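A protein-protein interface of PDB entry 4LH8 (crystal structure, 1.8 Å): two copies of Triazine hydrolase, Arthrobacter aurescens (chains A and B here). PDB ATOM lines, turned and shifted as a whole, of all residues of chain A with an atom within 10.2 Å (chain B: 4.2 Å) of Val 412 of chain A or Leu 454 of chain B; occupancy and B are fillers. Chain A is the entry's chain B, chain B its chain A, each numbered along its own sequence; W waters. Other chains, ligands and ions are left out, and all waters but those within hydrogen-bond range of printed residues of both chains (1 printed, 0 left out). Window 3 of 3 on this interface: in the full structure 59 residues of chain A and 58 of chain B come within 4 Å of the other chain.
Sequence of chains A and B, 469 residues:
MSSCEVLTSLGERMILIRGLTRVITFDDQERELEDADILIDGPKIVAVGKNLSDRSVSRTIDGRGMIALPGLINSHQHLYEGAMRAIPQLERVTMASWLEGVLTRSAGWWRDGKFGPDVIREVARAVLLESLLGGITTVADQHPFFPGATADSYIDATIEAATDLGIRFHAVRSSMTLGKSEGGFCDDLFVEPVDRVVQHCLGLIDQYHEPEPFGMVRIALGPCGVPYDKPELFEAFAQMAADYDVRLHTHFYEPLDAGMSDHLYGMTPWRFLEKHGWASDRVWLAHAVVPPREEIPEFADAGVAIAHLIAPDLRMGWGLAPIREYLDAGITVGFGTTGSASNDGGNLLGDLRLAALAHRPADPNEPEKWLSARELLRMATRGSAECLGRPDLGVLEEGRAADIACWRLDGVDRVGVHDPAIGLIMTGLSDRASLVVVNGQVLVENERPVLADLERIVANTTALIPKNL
The guanidinium group (NE) of Arg 408 of chain A lies within salt-bridge range of the side-chain carboxylate (OD1) of Asp 410 of chain A, 2.9 Å away.
The side-chain carboxylate of Asp 413 of chain A is in hydrogen-bond range of the backbone NH of Leu 429 of chain A (2.7 Å).
CG1 of Val 458 of chain B touches O of Asp 410 of chain A, 3.3 Å away.
CG2 of Val 412 of chain A touches O of Ala 126 of chain B, at 3.5 Å.
Val 412 of chain A touches Leu 133 of chain B.
CB of Val 412 of chain A touches CD1 of Leu 454 of chain B, 3.7 Å away.
CG2 of Val 458 of chain B touches CB of Val 412 of chain A, 3.6 Å away.
Leu 133 of chain B touches Leu 429 of chain A.
Printed residues of chain B within 4 Å of Asp 410 of chain A: Val 458 (3.3 Å).
Gly 411 of chain A touches none of the printed residues of chain B.
Of chain B, only Ala 126 (3.5 Å), Leu 133 (3.7 Å), Leu 454 (3.7 Å) and Val 458 (3.6 Å) come within 4 Å of Val 412 of chain A.
Printed residues of chain B within 4 Å of Leu 429 of chain A: Leu 133.
Ala 126 of chain B touches just one residue of chain A: Val 412.
Of the printed residues of chain A, Leu 133 of chain B touches Val 412 (3.7 Å) and Leu 429 (3.7 Å).
No residue of chain A comes within 4 Å of Ala 452 of chain B.
No residue of chain A comes within 4 Å of Asp 453 of chain B.
Of chain A, only Val 412 (3.7 Å) comes within 4 Å of Leu 454 of chain B.
Arg 456 of chain B touches none of the printed residues of chain A.
No residue of chain A comes within 4 Å of Ile 457 of chain B.
Of the printed residues of chain A, Val 458 of chain B touches Asp 410 (3.3 Å) and Val 412 (3.6 Å).
The nearest printed residue of chain B that does not touch Val 412 of chain A is Leu 129 of chain B (4.4 Å).
Of the 14 printed residues of chain A, 3 touch a printed residue of chain B.
Printed residues of chain A that touch a printed residue of chain B: Asp 410, Val 412 and Leu 429.
Hydrophobic or aromatic side chains of chain A within 4 Å of the printed part of chain B: Val 412 and Leu 429.
Of the 12 printed residues of chain B, 4 touch a printed residue of chain A.
Hydrophobic or aromatic side chains of chain B within 4 Å of the printed part of chain A: Ala 126, Leu 133, Leu 454 and Val 458.
No position is printed for both chains.
Water W1 bridges the backbone carbonyl oxygen (O) of Val 412 of chain A and the backbone carbonyl oxygen (O) of Ala 126 of chain B.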
ATOM      1  N   ARG A 408      31.686 -10.737 -14.201  1.00  0.00           N
ATOM      2  CA  ARG A 408      30.630  -9.879 -13.669  1.00  0.00           C
ATOM      3  C   ARG A 408      31.186  -8.860 -12.687  1.00  0.00           C
ATOM      4  O   ARG A 408      32.116  -9.155 -11.933  1.00  0.00           O
ATOM      5  CB  ARG A 408      29.518 -10.706 -13.016  1.00  0.00           C
ATOM      6  CG  ARG A 408      28.744 -11.562 -14.022  1.00  0.00           C
ATOM      7  CD  ARG A 408      27.288 -11.697 -13.614  1.00  0.00           C
ATOM      8  NE  ARG A 408      26.579 -10.432 -13.797  1.00  0.00           N
ATOM      9  CZ  ARG A 408      26.004 -10.055 -14.936  1.00  0.00           C
ATOM     10  NH1 ARG A 408      26.045 -10.847 -16.001  1.00  0.00           N
ATOM     11  NH2 ARG A 408      25.381  -8.884 -15.008  1.00  0.00           N
ATOM     12  N   LEU A 409      30.609  -7.662 -12.709  1.00  0.00           N
ATOM     13  CA  LEU A 409      31.018  -6.564 -11.836  1.00  0.00           C
ATOM     14  C   LEU A 409      29.996  -6.266 -10.744  1.00  0.00           C
ATOM     15  O   LEU A 409      30.246  -5.434  -9.870  1.00  0.00           O
ATOM     16  CB  LEU A 409      31.216  -5.294 -12.663  1.00  0.00           C
ATOM     17  CG  LEU A 409      32.282  -5.352 -13.754  1.00  0.00           C
ATOM     18  CD1 LEU A 409      32.133  -4.168 -14.710  1.00  0.00           C
ATOM     19  CD2 LEU A 409      33.694  -5.421 -13.152  1.00  0.00           C
ATOM     20  N   ASP A 410      28.853  -6.941 -10.794  1.00  0.00           N
ATOM     21  CA  ASP A 410      27.720  -6.577  -9.949  1.00  0.00           C
ATOM     22  C   ASP A 410      27.523  -7.458  -8.716  1.00  0.00           C
ATOM     23  O   ASP A 410      26.414  -7.545  -8.191  1.00  0.00           O
ATOM     24  CB  ASP A 410      26.423  -6.545 -10.773  1.00  0.00           C
ATOM     25  CG  ASP A 410      26.136  -7.862 -11.495  1.00  0.00           C
ATOM     26  OD1 ASP A 410      26.921  -8.831 -11.359  1.00  0.00           O
ATOM     27  OD2 ASP A 410      25.102  -7.930 -12.196  1.00  0.00           O
ATOM     28  N   GLY A 411      28.589  -8.100  -8.247  1.00  0.00           N
ATOM     29  CA  GLY A 411      28.479  -8.980  -7.096  1.00  0.00           C
ATOM     30  C   GLY A 411      28.681  -8.195  -5.818  1.00  0.00           C
ATOM     31  O   GLY A 411      29.217  -7.097  -5.858  1.00  0.00           O
ATOM     32  N   VAL A 412      28.267  -8.747  -4.679  1.00  0.00           N
ATOM     33  CA  VAL A 412      28.358  -8.002  -3.428  1.00  0.00           C
ATOM     34  C   VAL A 412      29.813  -7.745  -3.041  1.00  0.00           C
ATOM     35  O   VAL A 412      30.120  -6.760  -2.364  1.00  0.00           O
ATOM     36  CB  VAL A 412      27.619  -8.720  -2.278  1.00  0.00           C
ATOM     37  CG1 VAL A 412      28.365  -9.983  -1.868  1.00  0.00           C
ATOM     38  CG2 VAL A 412      27.420  -7.765  -1.093  1.00  0.00           C
ATOM     39  N   ASP A 413      30.711  -8.623  -3.495  1.00  0.00           N
ATOM     40  CA  ASP A 413      32.135  -8.497  -3.193  1.00  0.00           C
ATOM     41  C   ASP A 413      32.865  -7.467  -4.065  1.00  0.00           C
ATOM     42  O   ASP A 413      34.068  -7.246  -3.894  1.00  0.00           O
ATOM     43  CB  ASP A 413      32.836  -9.870  -3.253  1.00  0.00           C
ATOM     44  CG  ASP A 413      32.603 -10.601  -4.573  1.00  0.00           C
ATOM     45  OD1 ASP A 413      31.585 -10.325  -5.245  1.00  0.00           O
ATOM     46  OD2 ASP A 413      33.439 -11.467  -4.928  1.00  0.00           O
ATOM     47  N   ARG A 414      32.145  -6.829  -4.991  1.00  0.00           N
ATOM     48  CA  ARG A 414      32.741  -5.768  -5.803  1.00  0.00           C
ATOM     49  C   ARG A 414      31.980  -4.443  -5.709  1.00  0.00           C
ATOM     50  O   ARG A 414      32.188  -3.539  -6.528  1.00  0.00           O
ATOM     51  CB  ARG A 414      32.905  -6.203  -7.267  1.00  0.00           C
ATOM     52  CG  ARG A 414      33.799  -7.448  -7.447  1.00  0.00           C
ATOM     53  CD  ARG A 414      34.146  -7.677  -8.916  1.00  0.00           C
ATOM     54  NE  ARG A 414      34.608  -9.040  -9.186  1.00  0.00           N
ATOM     55  CZ  ARG A 414      35.880  -9.431  -9.146  1.00  0.00           C
ATOM     56  NH1 ARG A 414      36.839  -8.567  -8.836  1.00  0.00           N
ATOM     57  NH2 ARG A 414      36.194 -10.692  -9.416  1.00  0.00           N
ATOM     58  N   VAL A 415      31.113  -4.327  -4.704  1.00  0.00           N
ATOM     59  CA  VAL A 415      30.423  -3.069  -4.434  1.00  0.00           C
ATOM     60  C   VAL A 415      31.455  -2.027  -4.011  1.00  0.00           C
ATOM     61  O   VAL A 415      32.353  -2.322  -3.227  1.00  0.00           O
ATOM     62  CB  VAL A 415      29.369  -3.229  -3.311  1.00  0.00           C
ATOM     63  CG1 VAL A 415      28.754  -1.876  -2.947  1.00  0.00           C
ATOM     64  CG2 VAL A 415      28.283  -4.220  -3.726  1.00  0.00           C
ATOM     65  N   GLY A 416      31.330  -0.811  -4.531  1.00  0.00           N
ATOM     66  CA  GLY A 416      32.237   0.260  -4.162  1.00  0.00           C
ATOM     67  C   GLY A 416      33.519   0.322  -4.971  1.00  0.00           C
ATOM     68  O   GLY A 416      34.405   1.131  -4.674  1.00  0.00           O
ATOM     69  N   VAL A 417      33.627  -0.537  -5.980  1.00  0.00           N
ATOM     70  CA  VAL A 417      34.756  -0.505  -6.907  1.00  0.00           C
ATOM     71  C   VAL A 417      34.619   0.661  -7.874  1.00  0.00           C
ATOM     72  O   VAL A 417      33.609   0.780  -8.560  1.00  0.00           O
ATOM     73  CB  VAL A 417      34.846  -1.796  -7.735  1.00  0.00           C
ATOM     74  CG1 VAL A 417      35.748  -1.593  -8.965  1.00  0.00           C
ATOM     75  CG2 VAL A 417      35.343  -2.942  -6.866  1.00  0.00           C
ATOM     76  N   THR A 427      40.014  -6.860  -5.886  1.00  0.00           N
ATOM     77  CA  THR A 427      38.837  -7.259  -5.110  1.00  0.00           C
ATOM     78  C   THR A 427      38.348  -8.655  -5.478  1.00  0.00           C
ATOM     79  O   THR A 427      38.760  -9.227  -6.486  1.00  0.00           O
ATOM     80  CB  THR A 427      37.647  -6.270  -5.324  1.00  0.00           C
ATOM     81  OG1 THR A 427      37.183  -6.363  -6.678  1.00  0.00           O
ATOM     82  CG2 THR A 427      38.077  -4.820  -5.026  1.00  0.00           C
ATOM     83  N   GLY A 428      37.473  -9.212  -4.650  1.00  0.00           N
ATOM     84  CA  GLY A 428      36.713 -10.380  -5.064  1.00  0.00           C
ATOM     85  C   GLY A 428      36.907 -11.599  -4.198  1.00  0.00           C
ATOM     86  O   GLY A 428      37.995 -11.819  -3.652  1.00  0.00           O
ATOM     87  N   LEU A 429      35.842 -12.385  -4.071  1.00  0.00           N
ATOM     88  CA  LEU A 429      35.905 -13.686  -3.434  1.00  0.00           C
ATOM     89  C   LEU A 429      36.202 -14.796  -4.441  1.00  0.00           C
ATOM     90  O   LEU A 429      36.444 -15.939  -4.055  1.00  0.00           O
ATOM     91  CB  LEU A 429      34.580 -13.997  -2.732  1.00  0.00           C
ATOM     92  CG  LEU A 429      34.276 -13.190  -1.465  1.00  0.00           C
ATOM     93  CD1 LEU A 429      32.855 -13.457  -0.985  1.00  0.00           C
ATOM     94  CD2 LEU A 429      35.281 -13.527  -0.377  1.00  0.00           C
ATOM     95  N   SER A 430      36.192 -14.465  -5.727  1.00  0.00           N
ATOM     96  CA  SER A 430      36.258 -15.494  -6.759  1.00  0.00           C
ATOM     97  C   SER A 430      36.786 -14.946  -8.078  1.00  0.00           C
ATOM     98  O   SER A 430      36.406 -13.856  -8.494  1.00  0.00           O
ATOM     99  CB  SER A 430      34.862 -16.085  -6.987  1.00  0.00           C
ATOM    100  OG  SER A 430      34.853 -16.970  -8.099  1.00  0.00           O
ATOM    101  N   ALA B 126      27.040  -4.605   3.109  1.00  0.00           N
ATOM    102  CA  ALA B 126      27.641  -5.277   1.956  1.00  0.00           C
ATOM    103  C   ALA B 126      28.947  -5.979   2.309  1.00  0.00           C
ATOM    104  O   ALA B 126      29.153  -7.134   1.918  1.00  0.00           O
ATOM    105  CB  ALA B 126      27.873  -4.292   0.815  1.00  0.00           C
ATOM    106  N   LEU B 129      28.250  -8.923   4.506  1.00  0.00           N
ATOM    107  CA  LEU B 129      27.673 -10.035   3.759  1.00  0.00           C
ATOM    108  C   LEU B 129      28.755 -10.721   2.931  1.00  0.00           C
ATOM    109  O   LEU B 129      28.827 -11.950   2.870  1.00  0.00           O
ATOM    110  CB  LEU B 129      26.527  -9.555   2.855  1.00  0.00           C
ATOM    111  CG  LEU B 129      25.838 -10.662   2.046  1.00  0.00           C
ATOM    112  CD1 LEU B 129      25.414 -11.784   2.975  1.00  0.00           C
ATOM    113  CD2 LEU B 129      24.626 -10.108   1.297  1.00  0.00           C
ATOM    114  N   LEU B 133      30.036 -14.701   3.180  1.00  0.00           N
ATOM    115  CA  LEU B 133      30.205 -15.484   1.962  1.00  0.00           C
ATOM    116  C   LEU B 133      31.628 -16.019   1.799  1.00  0.00           C
ATOM    117  O   LEU B 133      31.851 -17.007   1.090  1.00  0.00           O
ATOM    118  CB  LEU B 133      29.796 -14.660   0.751  1.00  0.00           C
ATOM    119  CG  LEU B 133      28.298 -14.358   0.677  1.00  0.00           C
ATOM    120  CD1 LEU B 133      28.036 -13.441  -0.502  1.00  0.00           C
ATOM    121  CD2 LEU B 133      27.496 -15.653   0.549  1.00  0.00           C
ATOM    122  N   ARG B 448      25.220 -19.275  -1.107  1.00  0.00           N
ATOM    123  CA  ARG B 448      24.250 -18.185  -1.085  1.00  0.00           C
ATOM    124  C   ARG B 448      23.641 -17.953   0.287  1.00  0.00           C
ATOM    125  O   ARG B 448      23.438 -18.889   1.058  1.00  0.00           O
ATOM    126  CB  ARG B 448      23.151 -18.391  -2.133  1.00  0.00           C
ATOM    127  CG  ARG B 448      23.582 -18.004  -3.545  1.00  0.00           C
ATOM    128  CD  ARG B 448      22.398 -17.937  -4.496  1.00  0.00           C
ATOM    129  NE  ARG B 448      21.407 -16.938  -4.092  1.00  0.00           N
ATOM    130  CZ  ARG B 448      21.211 -15.780  -4.715  1.00  0.00           C
ATOM    131  NH1 ARG B 448      20.278 -14.943  -4.277  1.00  0.00           N
ATOM    132  NH2 ARG B 448      21.938 -15.459  -5.783  1.00  0.00           N
ATOM    133  N   PRO B 449      23.350 -16.685   0.594  1.00  0.00           N
ATOM    134  CA  PRO B 449      22.720 -16.295   1.858  1.00  0.00           C
ATOM    135  C   PRO B 449      21.351 -16.951   1.987  1.00  0.00           C
ATOM    136  O   PRO B 449      20.616 -17.027   1.006  1.00  0.00           O
ATOM    137  CB  PRO B 449      22.560 -14.780   1.720  1.00  0.00           C
ATOM    138  CG  PRO B 449      23.537 -14.373   0.673  1.00  0.00           C
ATOM    139  CD  PRO B 449      23.654 -15.529  -0.263  1.00  0.00           C
ATOM    140  N   ALA B 452      19.436 -13.458   4.110  1.00  0.00           N
ATOM    141  CA  ALA B 452      19.582 -12.154   3.469  1.00  0.00           C
ATOM    142  C   ALA B 452      19.237 -12.220   1.979  1.00  0.00           C
ATOM    143  O   ALA B 452      19.382 -13.270   1.358  1.00  0.00           O
ATOM    144  CB  ALA B 452      20.990 -11.606   3.678  1.00  0.00           C
ATOM    145  N   ASP B 453      18.763 -11.099   1.430  1.00  0.00           N
ATOM    146  CA  ASP B 453      18.472 -10.977  -0.006  1.00  0.00           C
ATOM    147  C   ASP B 453      19.682 -10.363  -0.691  1.00  0.00           C
ATOM    148  O   ASP B 453      19.862  -9.144  -0.682  1.00  0.00           O
ATOM    149  CB  ASP B 453      17.233 -10.103  -0.243  1.00  0.00           C
ATOM    150  CG  ASP B 453      16.777 -10.089  -1.706  1.00  0.00           C
ATOM    151  OD1 ASP B 453      17.620 -10.220  -2.627  1.00  0.00           O
ATOM    152  OD2 ASP B 453      15.559  -9.926  -1.933  1.00  0.00           O
ATOM    153  N   LEU B 454      20.513 -11.226  -1.269  1.00  0.00           N
ATOM    154  CA  LEU B 454      21.774 -10.827  -1.888  1.00  0.00           C
ATOM    155  C   LEU B 454      21.612  -9.738  -2.948  1.00  0.00           C
ATOM    156  O   LEU B 454      22.268  -8.692  -2.888  1.00  0.00           O
ATOM    157  CB  LEU B 454      22.456 -12.051  -2.509  1.00  0.00           C
ATOM    158  CG  LEU B 454      23.807 -11.837  -3.189  1.00  0.00           C
ATOM    159  CD1 LEU B 454      24.742 -11.112  -2.249  1.00  0.00           C
ATOM    160  CD2 LEU B 454      24.396 -13.180  -3.605  1.00  0.00           C
ATOM    161  N   GLU B 455      20.748  -9.991  -3.926  1.00  0.00           N
ATOM    162  CA  GLU B 455      20.562  -9.059  -5.031  1.00  0.00           C
ATOM    163  C   GLU B 455      20.058  -7.700  -4.553  1.00  0.00           C
ATOM    164  O   GLU B 455      20.475  -6.663  -5.056  1.00  0.00           O
ATOM    165  CB  GLU B 455      19.606  -9.646  -6.075  1.00  0.00           C
ATOM    166  CG  GLU B 455      20.219 -10.741  -6.945  1.00  0.00           C
ATOM    167  CD  GLU B 455      20.331 -12.098  -6.251  1.00  0.00           C
ATOM    168  OE1 GLU B 455      19.601 -12.359  -5.266  1.00  0.00           O
ATOM    169  OE2 GLU B 455      21.155 -12.917  -6.705  1.00  0.00           O
ATOM    170  N   ARG B 456      19.156  -7.698  -3.582  1.00  0.00           N
ATOM    171  CA  ARG B 456      18.595  -6.436  -3.121  1.00  0.00           C
ATOM    172  C   ARG B 456      19.626  -5.610  -2.352  1.00  0.00           C
ATOM    173  O   ARG B 456      19.671  -4.384  -2.463  1.00  0.00           O
ATOM    174  CB  ARG B 456      17.339  -6.654  -2.275  1.00  0.00           C
ATOM    175  CG  ARG B 456      16.618  -5.347  -1.973  1.00  0.00           C
ATOM    176  CD  ARG B 456      15.333  -5.516  -1.174  1.00  0.00           C
ATOM    177  NE  ARG B 456      14.631  -4.235  -1.074  1.00  0.00           N
ATOM    178  CZ  ARG B 456      14.874  -3.318  -0.142  1.00  0.00           C
ATOM    179  NH1 ARG B 456      15.794  -3.541   0.787  1.00  0.00           N
ATOM    180  NH2 ARG B 456      14.197  -2.176  -0.133  1.00  0.00           N
ATOM    181  N   ILE B 457      20.465  -6.294  -1.581  1.00  0.00           N
ATOM    182  CA  ILE B 457      21.496  -5.623  -0.797  1.00  0.00           C
ATOM    183  C   ILE B 457      22.533  -4.998  -1.715  1.00  0.00           C
ATOM    184  O   ILE B 457      22.991  -3.882  -1.480  1.00  0.00           O
ATOM    185  CB  ILE B 457      22.166  -6.591   0.205  1.00  0.00           C
ATOM    186  CG1 ILE B 457      21.214  -6.853   1.382  1.00  0.00           C
ATOM    187  CG2 ILE B 457      23.501  -6.020   0.698  1.00  0.00           C
ATOM    188  CD1 ILE B 457      21.604  -8.011   2.281  1.00  0.00           C
ATOM    189  N   VAL B 458      22.893  -5.715  -2.776  1.00  0.00           N
ATOM    190  CA  VAL B 458      23.839  -5.181  -3.740  1.00  0.00           C
ATOM    191  C   VAL B 458      23.282  -3.919  -4.391  1.00  0.00           C
ATOM    192  O   VAL B 458      23.964  -2.899  -4.482  1.00  0.00           O
ATOM    193  CB  VAL B 458      24.177  -6.205  -4.833  1.00  0.00           C
ATOM    194  CG1 VAL B 458      25.023  -5.558  -5.917  1.00  0.00           C
ATOM    195  CG2 VAL B 458      24.892  -7.403  -4.224  1.00  0.00           C
HETATM  196  O   HOH W   1      31.474  -5.775  -0.106  1.00  0.00           O
